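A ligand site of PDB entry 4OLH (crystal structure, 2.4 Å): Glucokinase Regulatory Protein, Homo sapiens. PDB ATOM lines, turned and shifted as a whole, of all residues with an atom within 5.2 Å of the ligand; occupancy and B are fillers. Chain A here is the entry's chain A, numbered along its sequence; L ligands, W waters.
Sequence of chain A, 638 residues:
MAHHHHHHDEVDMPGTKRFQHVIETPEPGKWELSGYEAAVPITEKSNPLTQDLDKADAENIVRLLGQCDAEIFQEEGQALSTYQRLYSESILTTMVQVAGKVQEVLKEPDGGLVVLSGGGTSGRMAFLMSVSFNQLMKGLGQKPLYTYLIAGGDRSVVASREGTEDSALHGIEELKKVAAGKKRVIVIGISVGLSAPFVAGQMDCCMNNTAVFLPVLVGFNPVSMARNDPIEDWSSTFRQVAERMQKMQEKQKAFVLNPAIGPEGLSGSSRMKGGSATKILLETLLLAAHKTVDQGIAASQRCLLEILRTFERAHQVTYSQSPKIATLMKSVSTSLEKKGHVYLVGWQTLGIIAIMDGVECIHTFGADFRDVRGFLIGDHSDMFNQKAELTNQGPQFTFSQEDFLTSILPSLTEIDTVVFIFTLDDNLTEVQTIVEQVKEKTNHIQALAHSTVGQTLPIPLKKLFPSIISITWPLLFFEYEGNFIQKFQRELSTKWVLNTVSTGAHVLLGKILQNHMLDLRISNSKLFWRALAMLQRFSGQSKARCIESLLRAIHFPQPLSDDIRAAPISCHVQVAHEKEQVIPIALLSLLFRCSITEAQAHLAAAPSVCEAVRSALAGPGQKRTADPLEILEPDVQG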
ATOM      1  N   ILE A  23      18.567  10.975  20.294  1.00  0.00           N
ATOM      2  CA  ILE A  23      18.756  11.476  21.639  1.00  0.00           C
ATOM      3  C   ILE A  23      19.849  10.644  22.290  1.00  0.00           C
ATOM      4  O   ILE A  23      19.842   9.401  22.141  1.00  0.00           O
ATOM      5  CB  ILE A  23      17.487  11.313  22.520  1.00  0.00           C
ATOM      6  CG1 ILE A  23      16.206  11.897  21.868  1.00  0.00           C
ATOM      7  CG2 ILE A  23      17.712  11.902  23.920  1.00  0.00           C
ATOM      8  CD1 ILE A  23      16.277  13.351  21.469  1.00  0.00           C
ATOM      9  N   TRP A  31      16.357   8.196  33.158  1.00  0.00           N
ATOM     10  CA  TRP A  31      15.646   8.038  31.874  1.00  0.00           C
ATOM     11  C   TRP A  31      14.408   8.924  31.771  1.00  0.00           C
ATOM     12  O   TRP A  31      14.170   9.549  30.722  1.00  0.00           O
ATOM     13  CB  TRP A  31      15.283   6.588  31.596  1.00  0.00           C
ATOM     14  CG  TRP A  31      16.462   5.754  31.128  1.00  0.00           C
ATOM     15  CD1 TRP A  31      17.439   5.241  31.920  1.00  0.00           C
ATOM     16  CD2 TRP A  31      16.781   5.358  29.785  1.00  0.00           C
ATOM     17  NE1 TRP A  31      18.352   4.554  31.152  1.00  0.00           N
ATOM     18  CE2 TRP A  31      17.972   4.603  29.847  1.00  0.00           C
ATOM     19  CE3 TRP A  31      16.168   5.563  28.538  1.00  0.00           C
ATOM     20  CZ2 TRP A  31      18.566   4.049  28.702  1.00  0.00           C
ATOM     21  CZ3 TRP A  31      16.767   5.022  27.403  1.00  0.00           C
ATOM     22  CH2 TRP A  31      17.959   4.277  27.492  1.00  0.00           C
ATOM     23  N   TYR A  36      13.978  11.801  28.040  1.00  0.00           N
ATOM     24  CA  TYR A  36      14.102  10.835  26.942  1.00  0.00           C
ATOM     25  C   TYR A  36      12.761  10.153  26.775  1.00  0.00           C
ATOM     26  O   TYR A  36      12.204  10.174  25.719  1.00  0.00           O
ATOM     27  CB  TYR A  36      15.168   9.790  27.253  1.00  0.00           C
ATOM     28  CG  TYR A  36      15.488   8.804  26.167  1.00  0.00           C
ATOM     29  CD1 TYR A  36      14.740   7.648  25.985  1.00  0.00           C
ATOM     30  CD2 TYR A  36      16.581   8.984  25.350  1.00  0.00           C
ATOM     31  CE1 TYR A  36      15.067   6.708  25.018  1.00  0.00           C
ATOM     32  CE2 TYR A  36      16.910   8.061  24.369  1.00  0.00           C
ATOM     33  CZ  TYR A  36      16.157   6.916  24.206  1.00  0.00           C
ATOM     34  OH  TYR A  36      16.491   6.006  23.234  1.00  0.00           O
ATOM     35  N   GLU A  37      12.263   9.567  27.863  1.00  0.00           N
ATOM     36  CA  GLU A  37      10.980   8.851  27.895  1.00  0.00           C
ATOM     37  C   GLU A  37       9.823   9.682  27.301  1.00  0.00           C
ATOM     38  O   GLU A  37       9.069   9.187  26.469  1.00  0.00           O
ATOM     39  CB  GLU A  37      10.679   8.495  29.362  1.00  0.00           C
ATOM     40  CG  GLU A  37      10.430   7.043  29.731  1.00  0.00           C
ATOM     41  CD  GLU A  37      11.373   6.042  29.098  1.00  0.00           C
ATOM     42  OE1 GLU A  37      12.222   5.462  29.823  1.00  0.00           O
ATOM     43  OE2 GLU A  37      11.188   5.777  27.889  1.00  0.00           O
ATOM     44  N   ALA A  39      10.137  11.884  25.037  1.00  0.00           N
ATOM     45  CA  ALA A  39      10.341  11.980  23.608  1.00  0.00           C
ATOM     46  C   ALA A  39       9.944  10.693  22.851  1.00  0.00           C
ATOM     47  O   ALA A  39       9.853  10.716  21.610  1.00  0.00           O
ATOM     48  CB  ALA A  39      11.807  12.308  23.328  1.00  0.00           C
ATOM     49  N   VAL A  40       9.720   9.581  23.573  1.00  0.00           N
ATOM     50  CA  VAL A  40       9.342   8.335  22.883  1.00  0.00           C
ATOM     51  C   VAL A  40       7.876   8.385  22.485  1.00  0.00           C
ATOM     52  O   VAL A  40       7.004   8.445  23.327  1.00  0.00           O
ATOM     53  CB  VAL A  40       9.657   7.065  23.691  1.00  0.00           C
ATOM     54  CG1 VAL A  40       9.332   5.784  22.898  1.00  0.00           C
ATOM     55  CG2 VAL A  40      11.128   7.048  24.114  1.00  0.00           C
ATOM     56  N   PRO A  41       7.576   8.341  21.182  1.00  0.00           N
ATOM     57  CA  PRO A  41       6.146   8.389  20.859  1.00  0.00           C
ATOM     58  C   PRO A  41       5.395   7.265  21.484  1.00  0.00           C
ATOM     59  O   PRO A  41       5.939   6.177  21.717  1.00  0.00           O
ATOM     60  CB  PRO A  41       6.125   8.220  19.339  1.00  0.00           C
ATOM     61  CG  PRO A  41       7.490   8.695  18.894  1.00  0.00           C
ATOM     62  CD  PRO A  41       8.413   8.236  19.979  1.00  0.00           C
ATOM     63  N   THR A  43       3.428   5.224  20.342  1.00  0.00           N
ATOM     64  CA  THR A  43       3.337   4.024  19.535  1.00  0.00           C
ATOM     65  C   THR A  43       4.596   3.207  19.626  1.00  0.00           C
ATOM     66  O   THR A  43       4.577   1.986  19.424  1.00  0.00           O
ATOM     67  CB  THR A  43       2.989   4.328  18.063  1.00  0.00           C
ATOM     68  OG1 THR A  43       4.058   5.026  17.403  1.00  0.00           O
ATOM     69  CG2 THR A  43       1.685   5.134  17.971  1.00  0.00           C
ATOM     70  N   GLU A  44       5.672   3.854  20.026  1.00  0.00           N
ATOM     71  CA  GLU A  44       6.974   3.215  20.106  1.00  0.00           C
ATOM     72  C   GLU A  44       7.334   2.714  21.472  1.00  0.00           C
ATOM     73  O   GLU A  44       8.281   1.973  21.618  1.00  0.00           O
ATOM     74  CB  GLU A  44       8.052   4.183  19.607  1.00  0.00           C
ATOM     75  CG  GLU A  44       7.631   4.789  18.264  1.00  0.00           C
ATOM     76  CD  GLU A  44       7.264   3.742  17.246  1.00  0.00           C
ATOM     77  OE1 GLU A  44       8.141   2.859  16.987  1.00  0.00           O
ATOM     78  OE2 GLU A  44       6.108   3.789  16.734  1.00  0.00           O
ATOM     79  N   LYS A  45       6.570   3.096  22.472  1.00  0.00           N
ATOM     80  CA  LYS A  45       6.879   2.735  23.841  1.00  0.00           C
ATOM     81  C   LYS A  45       6.818   1.254  24.189  1.00  0.00           C
ATOM     82  O   LYS A  45       6.263   0.422  23.462  1.00  0.00           O
ATOM     83  CB  LYS A  45       5.971   3.504  24.813  1.00  0.00           C
ATOM     84  CG  LYS A  45       6.198   5.023  24.897  1.00  0.00           C
ATOM     85  CD  LYS A  45       5.443   5.569  26.129  1.00  0.00           C
ATOM     86  CE  LYS A  45       5.066   7.056  26.022  1.00  0.00           C
ATOM     87  NZ  LYS A  45       6.272   7.948  25.926  1.00  0.00           N
ATOM     88  N   SER A  46       7.447   0.968  25.321  1.00  0.00           N
ATOM     89  CA  SER A  46       7.280  -0.278  26.062  1.00  0.00           C
ATOM     90  C   SER A  46       5.968  -0.191  26.841  1.00  0.00           C
ATOM     91  O   SER A  46       5.813   0.697  27.652  1.00  0.00           O
ATOM     92  CB  SER A  46       8.457  -0.462  27.066  1.00  0.00           C
ATOM     93  OG  SER A  46       8.204  -1.466  28.036  1.00  0.00           O
ATOM     94  N   GLY A 193       2.262   4.927  13.353  1.00  0.00           N
ATOM     95  CA  GLY A 193       3.241   5.684  14.034  1.00  0.00           C
ATOM     96  C   GLY A 193       3.351   7.104  13.517  1.00  0.00           C
ATOM     97  O   GLY A 193       4.096   7.867  14.071  1.00  0.00           O
ATOM     98  N   LEU A 194       2.562   7.469  12.506  1.00  0.00           N
ATOM     99  CA  LEU A 194       2.713   8.773  11.797  1.00  0.00           C
ATOM    100  C   LEU A 194       4.208   8.858  11.352  1.00  0.00           C
ATOM    101  O   LEU A 194       4.984   9.716  11.739  1.00  0.00           O
ATOM    102  CB  LEU A 194       2.294   9.944  12.664  1.00  0.00           C
ATOM    103  CG  LEU A 194       0.862  10.059  13.203  1.00  0.00           C
ATOM    104  CD1 LEU A 194       0.640  11.420  13.858  1.00  0.00           C
ATOM    105  CD2 LEU A 194      -0.230   9.862  12.160  1.00  0.00           C
ATOM    106  N   SER A 195       4.567   7.871  10.553  1.00  0.00           N
ATOM    107  CA  SER A 195       5.936   7.488  10.341  1.00  0.00           C
ATOM    108  C   SER A 195       6.329   7.224   8.890  1.00  0.00           C
ATOM    109  O   SER A 195       7.482   7.393   8.567  1.00  0.00           O
ATOM    110  CB  SER A 195       6.163   6.189  11.105  1.00  0.00           C
ATOM    111  OG  SER A 195       7.372   5.562  10.707  1.00  0.00           O
ATOM    112  N   ASN A 221      -0.396   8.736  17.242  1.00  0.00           N
ATOM    113  CA  ASN A 221       0.471   9.602  18.030  1.00  0.00           C
ATOM    114  C   ASN A 221      -0.019  11.031  17.898  1.00  0.00           C
ATOM    115  O   ASN A 221      -0.610  11.394  16.886  1.00  0.00           O
ATOM    116  CB  ASN A 221       1.908   9.593  17.549  1.00  0.00           C
ATOM    117  CG  ASN A 221       2.671   8.330  17.921  1.00  0.00           C
ATOM    118  OD1 ASN A 221       2.693   7.905  19.071  1.00  0.00           O
ATOM    119  ND2 ASN A 221       3.358   7.770  16.948  1.00  0.00           N
ATOM    120  N   MET A 225       4.545  14.189  18.374  1.00  0.00           N
ATOM    121  CA  MET A 225       5.416  13.023  18.392  1.00  0.00           C
ATOM    122  C   MET A 225       5.528  12.352  17.021  1.00  0.00           C
ATOM    123  O   MET A 225       6.032  11.254  16.941  1.00  0.00           O
ATOM    124  CB  MET A 225       4.924  12.003  19.412  1.00  0.00           C
ATOM    125  CG  MET A 225       4.900  12.434  20.886  1.00  0.00           C
ATOM    126  SD  MET A 225       3.838  11.246  21.727  1.00  0.00           S
ATOM    127  CE  MET A 225       4.375  11.338  23.439  1.00  0.00           C
ATOM    128  N   ALA A 226       5.036  12.992  15.957  1.00  0.00           N
ATOM    129  CA  ALA A 226       5.175  12.473  14.602  1.00  0.00           C
ATOM    130  C   ALA A 226       6.622  12.355  14.223  1.00  0.00           C
ATOM    131  O   ALA A 226       7.395  13.186  14.597  1.00  0.00           O
ATOM    132  CB  ALA A 226       4.486  13.372  13.600  1.00  0.00           C
ATOM    133  N   ARG A 227       6.964  11.361  13.413  1.00  0.00           N
ATOM    134  CA  ARG A 227       8.352  11.140  12.970  1.00  0.00           C
ATOM    135  C   ARG A 227       8.976  12.386  12.319  1.00  0.00           C
ATOM    136  O   ARG A 227       8.330  13.086  11.544  1.00  0.00           O
ATOM    137  CB  ARG A 227       8.390   9.937  12.037  1.00  0.00           C
ATOM    138  CG  ARG A 227       9.759   9.484  11.685  1.00  0.00           C
ATOM    139  CD  ARG A 227       9.731   8.099  11.076  1.00  0.00           C
ATOM    140  NE  ARG A 227      11.035   7.697  10.586  1.00  0.00           N
ATOM    141  CZ  ARG A 227      11.304   6.582   9.910  1.00  0.00           C
ATOM    142  NH1 ARG A 227      10.366   5.713   9.665  1.00  0.00           N
ATOM    143  NH2 ARG A 227      12.523   6.333   9.494  1.00  0.00           N
ATOM    144  N   ASN A 228      10.240  12.649  12.668  1.00  0.00           N
ATOM    145  CA  ASN A 228      10.928  13.876  12.294  1.00  0.00           C
ATOM    146  C   ASN A 228      12.346  13.697  11.788  1.00  0.00           C
ATOM    147  O   ASN A 228      13.005  14.667  11.606  1.00  0.00           O
ATOM    148  CB  ASN A 228      10.930  14.838  13.493  1.00  0.00           C
ATOM    149  CG  ASN A 228      11.026  16.319  13.075  1.00  0.00           C
ATOM    150  OD1 ASN A 228      10.434  16.789  12.112  1.00  0.00           O
ATOM    151  ND2 ASN A 228      11.794  17.044  13.832  1.00  0.00           N
ATOM    152  N   ASP A 229      12.822  12.495  11.537  1.00  0.00           N
ATOM    153  CA  ASP A 229      14.124  12.320  10.853  1.00  0.00           C
ATOM    154  C   ASP A 229      13.912  12.425   9.351  1.00  0.00           C
ATOM    155  O   ASP A 229      12.906  11.971   8.866  1.00  0.00           O
ATOM    156  CB  ASP A 229      14.816  10.965  11.174  1.00  0.00           C
ATOM    157  CG  ASP A 229      13.928   9.770  10.885  1.00  0.00           C
ATOM    158  OD1 ASP A 229      12.772   9.832  11.377  1.00  0.00           O
ATOM    159  OD2 ASP A 229      14.353   8.776  10.215  1.00  0.00           O
ATOM    160  N   SER A 267       6.487  -4.089  21.960  1.00  0.00           N
ATOM    161  CA  SER A 267       6.819  -2.714  21.578  1.00  0.00           C
ATOM    162  C   SER A 267       6.981  -2.560  20.083  1.00  0.00           C
ATOM    163  O   SER A 267       7.750  -3.281  19.479  1.00  0.00           O
ATOM    164  CB  SER A 267       8.066  -2.169  22.258  1.00  0.00           C
ATOM    165  OG  SER A 267       8.230  -2.722  23.526  1.00  0.00           O
ATOM    166  N   HIS A 516      10.087  -6.867  24.234  1.00  0.00           N
ATOM    167  CA  HIS A 516      10.751  -6.417  23.016  1.00  0.00           C
ATOM    168  C   HIS A 516      11.120  -7.612  22.138  1.00  0.00           C
ATOM    169  O   HIS A 516      11.584  -8.657  22.632  1.00  0.00           O
ATOM    170  CB  HIS A 516      12.033  -5.652  23.390  1.00  0.00           C
ATOM    171  CG  HIS A 516      11.780  -4.385  24.158  1.00  0.00           C
ATOM    172  ND1 HIS A 516      11.212  -3.265  23.588  1.00  0.00           N
ATOM    173  CD2 HIS A 516      12.015  -4.073  25.460  1.00  0.00           C
ATOM    174  CE1 HIS A 516      11.106  -2.315  24.494  1.00  0.00           C
ATOM    175  NE2 HIS A 516      11.602  -2.766  25.636  1.00  0.00           N
ATOM    176  N   SER A 525      14.198   1.843   7.514  1.00  0.00           N
ATOM    177  CA  SER A 525      14.788   2.798   8.435  1.00  0.00           C
ATOM    178  C   SER A 525      14.195   2.761   9.892  1.00  0.00           C
ATOM    179  O   SER A 525      14.922   2.839  10.886  1.00  0.00           O
ATOM    180  CB  SER A 525      14.725   4.209   7.870  1.00  0.00           C
ATOM    181  OG  SER A 525      13.446   4.562   7.398  1.00  0.00           O
ATOM    182  N   LYS A 526      12.889   2.622   9.991  1.00  0.00           N
ATOM    183  CA  LYS A 526      12.225   2.625  11.300  1.00  0.00           C
ATOM    184  C   LYS A 526      12.749   1.497  12.202  1.00  0.00           C
ATOM    185  O   LYS A 526      13.073   1.699  13.390  1.00  0.00           O
ATOM    186  CB  LYS A 526      10.703   2.582  11.131  1.00  0.00           C
ATOM    187  CG  LYS A 526       9.924   2.333  12.414  1.00  0.00           C
ATOM    188  CD  LYS A 526       8.418   2.373  12.143  1.00  0.00           C
ATOM    189  CE  LYS A 526       7.930   1.090  11.481  1.00  0.00           C
ATOM    190  NZ  LYS A 526       6.490   1.181  11.157  1.00  0.00           N
ATOM    191  N   TRP A 529      16.024   2.406  13.273  1.00  0.00           N
ATOM    192  CA  TRP A 529      16.073   3.316  14.414  1.00  0.00           C
ATOM    193  C   TRP A 529      15.690   2.601  15.697  1.00  0.00           C
ATOM    194  O   TRP A 529      16.226   2.887  16.757  1.00  0.00           O
ATOM    195  CB  TRP A 529      15.216   4.542  14.175  1.00  0.00           C
ATOM    196  CG  TRP A 529      15.748   5.379  13.064  1.00  0.00           C
ATOM    197  CD1 TRP A 529      15.100   5.736  11.928  1.00  0.00           C
ATOM    198  CD2 TRP A 529      17.019   5.988  13.020  1.00  0.00           C
ATOM    199  NE1 TRP A 529      15.898   6.538  11.181  1.00  0.00           N
ATOM    200  CE2 TRP A 529      17.101   6.698  11.815  1.00  0.00           C
ATOM    201  CE3 TRP A 529      18.129   5.984  13.897  1.00  0.00           C
ATOM    202  CZ2 TRP A 529      18.229   7.420  11.439  1.00  0.00           C
ATOM    203  CZ3 TRP A 529      19.260   6.684  13.530  1.00  0.00           C
ATOM    204  CH2 TRP A 529      19.299   7.394  12.297  1.00  0.00           C
ATOM    205  N   ARG A 530      14.830   1.624  15.588  1.00  0.00           N
ATOM    206  CA  ARG A 530      14.474   0.798  16.731  1.00  0.00           C
ATOM    207  C   ARG A 530      15.666  -0.052  17.240  1.00  0.00           C
ATOM    208  O   ARG A 530      15.951  -0.129  18.439  1.00  0.00           O
ATOM    209  CB  ARG A 530      13.265  -0.050  16.340  1.00  0.00           C
ATOM    210  CG  ARG A 530      12.628  -0.890  17.450  1.00  0.00           C
ATOM    211  CD  ARG A 530      11.127  -1.015  17.174  1.00  0.00           C
ATOM    212  NE  ARG A 530      10.514  -1.130  18.442  1.00  0.00           N
ATOM    213  CZ  ARG A 530       9.750  -0.243  19.043  1.00  0.00           C
ATOM    214  NH1 ARG A 530       9.319   0.866  18.485  1.00  0.00           N
ATOM    215  NH2 ARG A 530       9.364  -0.527  20.243  1.00  0.00           N
ATOM    216  N   ALA A 533      17.893   2.161  19.235  1.00  0.00           N
ATOM    217  CA  ALA A 533      17.271   2.441  20.503  1.00  0.00           C
ATOM    218  C   ALA A 533      17.349   1.234  21.406  1.00  0.00           C
ATOM    219  O   ALA A 533      17.568   1.389  22.602  1.00  0.00           O
ATOM    220  CB  ALA A 533      15.810   2.855  20.344  1.00  0.00           C
ATOM    221  N   MET A 534      17.101   0.049  20.860  1.00  0.00           N
ATOM    222  CA  MET A 534      17.205  -1.114  21.729  1.00  0.00           C
ATOM    223  C   MET A 534      18.622  -1.247  22.298  1.00  0.00           C
ATOM    224  O   MET A 534      18.777  -1.629  23.440  1.00  0.00           O
ATOM    225  CB  MET A 534      16.742  -2.369  21.047  1.00  0.00           C
ATOM    226  CG  MET A 534      15.233  -2.388  20.868  1.00  0.00           C
ATOM    227  SD  MET A 534      14.687  -4.012  20.362  1.00  0.00           S
ATOM    228  CE  MET A 534      15.168  -4.011  18.667  1.00  0.00           C
ATOM    229  N   ARG A 537      19.094   1.389  25.224  1.00  0.00           N
ATOM    230  CA  ARG A 537      18.290   0.988  26.370  1.00  0.00           C
ATOM    231  C   ARG A 537      18.876  -0.232  27.077  1.00  0.00           C
ATOM    232  O   ARG A 537      19.197  -0.135  28.244  1.00  0.00           O
ATOM    233  CB  ARG A 537      16.822   0.780  25.966  1.00  0.00           C
ATOM    234  CG  ARG A 537      15.925   0.046  26.979  1.00  0.00           C
ATOM    235  CD  ARG A 537      15.097   0.943  27.838  1.00  0.00           C
ATOM    236  NE  ARG A 537      14.227   1.816  27.059  1.00  0.00           N
ATOM    237  CZ  ARG A 537      13.571   2.854  27.550  1.00  0.00           C
ATOM    238  NH1 ARG A 537      13.650   3.183  28.831  1.00  0.00           N
ATOM    239  NH2 ARG A 537      12.845   3.610  26.742  1.00  0.00           N
HETATM  240  C1  LIG L   1       8.921   6.269  14.383  1.00  0.00           C
HETATM  241  C2  LIG L   1       7.746   6.896  14.711  1.00  0.00           C
HETATM  242  C3  LIG L   1       7.747   8.185  15.229  1.00  0.00           C
HETATM  243  N1  LIG L   1       6.595   8.790  15.534  1.00  0.00           N
HETATM  244  N2  LIG L   1       8.934   8.805  15.421  1.00  0.00           N
HETATM  245  C4  LIG L   1      10.080   8.212  15.135  1.00  0.00           C
HETATM  246  C5  LIG L   1      10.111   6.935  14.602  1.00  0.00           C
HETATM  247  S1  LIG L   1      11.631   6.178  14.254  1.00  0.00           S
HETATM  248  O1  LIG L   1      11.562   5.267  13.144  1.00  0.00           O
HETATM  249  O2  LIG L   1      12.669   7.227  13.983  1.00  0.00           O
HETATM  250  N3  LIG L   1      12.098   5.332  15.550  1.00  0.00           N
HETATM  251  C6  LIG L   1      10.975   4.513  15.994  1.00  0.00           C
HETATM  252  C7  LIG L   1      11.338   3.691  17.211  1.00  0.00           C
HETATM  253  C8  LIG L   1      12.476   6.252  16.602  1.00  0.00           C
HETATM  254  C9  LIG L   1      13.145   5.403  17.639  1.00  0.00           C
HETATM  255  N4  LIG L   1      12.206   4.411  18.148  1.00  0.00           N
HETATM  256  C10 LIG L   1      12.312   3.926  19.445  1.00  0.00           C
HETATM  257  N5  LIG L   1      12.175   2.607  19.552  1.00  0.00           N
HETATM  258  C11 LIG L   1      12.262   1.970  20.720  1.00  0.00           C
HETATM  259  C12 LIG L   1      12.553   2.630  21.907  1.00  0.00           C
HETATM  260  C13 LIG L   1      12.719   1.918  23.266  1.00  0.00           C
HETATM  261  C14 LIG L   1      11.365   1.633  23.918  1.00  0.00           C
HETATM  262  F1  LIG L   1      10.673   0.827  23.127  1.00  0.00           F
HETATM  263  F2  LIG L   1      10.795   2.806  24.117  1.00  0.00           F
HETATM  264  F3  LIG L   1      11.471   1.095  25.145  1.00  0.00           F
HETATM  265  C15 LIG L   1      13.554   0.665  23.176  1.00  0.00           C
HETATM  266  F4  LIG L   1      14.677   0.920  22.578  1.00  0.00           F
HETATM  267  F5  LIG L   1      12.993  -0.271  22.512  1.00  0.00           F
HETATM  268  F6  LIG L   1      13.806   0.233  24.415  1.00  0.00           F
HETATM  269  O3  LIG L   1      13.491   2.716  24.147  1.00  0.00           O
HETATM  270  C16 LIG L   1      12.691   4.003  21.816  1.00  0.00           C
HETATM  271  C17 LIG L   1      12.583   4.677  20.590  1.00  0.00           C
HETATM  272  C18 LIG L   1      12.754   6.075  20.633  1.00  0.00           C
HETATM  273  C19 LIG L   1      13.703   6.634  21.498  1.00  0.00           C
HETATM  274  C20 LIG L   1      13.826   8.023  21.570  1.00  0.00           C
HETATM  275  C21 LIG L   1      13.020   8.827  20.770  1.00  0.00           C
HETATM  276  N6  LIG L   1      12.107   8.262  19.966  1.00  0.00           N
HETATM  277  C22 LIG L   1      11.970   6.933  19.872  1.00  0.00           C
HETATM  278  O   HOH W   1       9.129  11.356  16.740  1.00  0.00           O
HETATM  279  O   HOH W   2      15.893   3.549  23.737  1.00  0.00           O
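O of Gly 193 is in hydrogen-bond range of N1 of the ligand (3.0 Å).
O of Met 225 lies within hydrogen-bond range of N1 of the ligand (2.9 Å).
NH2 of Arg 537 is in hydrogen-bond range of O3 of the ligand.
The backbone carbonyl oxygen (O) of Val 40 sits at hydrogen-bond distance from the side-chain amino group (NZ) of Lys 45 (2.7 Å).
OE2 of Glu 44 lies within hydrogen-bond range of OG1 of Thr 43.
The side-chain carboxylate of Glu 37 is in salt-bridge range of the guanidinium group of Arg 537, at 2.9 Å.
O of Gly 193 lies within hydrogen-bond range of ND2 of Asn 221, at 3.0 Å.
O of Ser 267 sits close to NH2 of Arg 530, 3.3 Å away.
The guanidinium group (NH2) of Arg 227 lies within hydrogen-bond range of the side-chain hydroxyl (OG) of Ser 525 (2.9 Å).
The side-chain hydroxyl (OG) of Ser 195 is in hydrogen-bond range of the guanidinium group (NH1) of Arg 227.
The side-chain carboxylate (OE1) of Glu 44 is in salt-bridge range of the guanidinium group (NH1) of Arg 530 (2.8 Å).
The backbone carbonyl oxygen of Glu 44 sits close to a fluorine (F1) of the ligand, 3.1 Å away.
The backbone NH (N) of Arg 227 lies close to a nitrogen (N1) of the ligand (3.4 Å).
NH2 of Arg 530 lies close to F1 of the ligand.
O of Ala 533 lies close to F4 of the ligand, 2.9 Å away.
The backbone NH of Met 534 sits close to a fluorine (F4) of the ligand, 3.1 Å away.
Tyr 36 touches the ligand (OH to C19, 3.3 Å).
Ala 39 touches the ligand.
CG1 of Val 40 touches F2 of the ligand, at 3.5 Å.
Pro 41 touches the ligand.
Lys 45 touches the ligand.
CB of Ser 46 touches F3 of the ligand, 3.9 Å away.
ND2 of Asn 221 touches N1 of the ligand, at 3.7 Å.
Ala 226 touches the ligand (C to N1, 3.8 Å).
OD1 of Asp 229 touches O2 of the ligand, at 3.7 Å.
His 516 touches the ligand (CE1 to F5, 3.4 Å).
Lys 526 touches the ligand (CA to O1, 3.3 Å).
Trp 529 touches the ligand (CB to N3, 3.5 Å).
20 residues have an atom within 4 Å of the ligand: Tyr 36, Ala 39, Val 40, Pro 41, Glu 44, Lys 45, Ser 46, Gly 193, Asn 221, Met 225, Ala 226, Arg 227, Asp 229, His 516, Lys 526, Trp 529, Arg 530, Ala 533, Met 534 and Arg 537.
Water W2 lies within hydrogen-bond range of an oxygen (O3) of the ligand (2.6 Å), the side-chain hydroxyl (OH) of Tyr 36 (2.6 Å) and the backbone carbonyl oxygen (O) of Ala 533 (3.0 Å).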
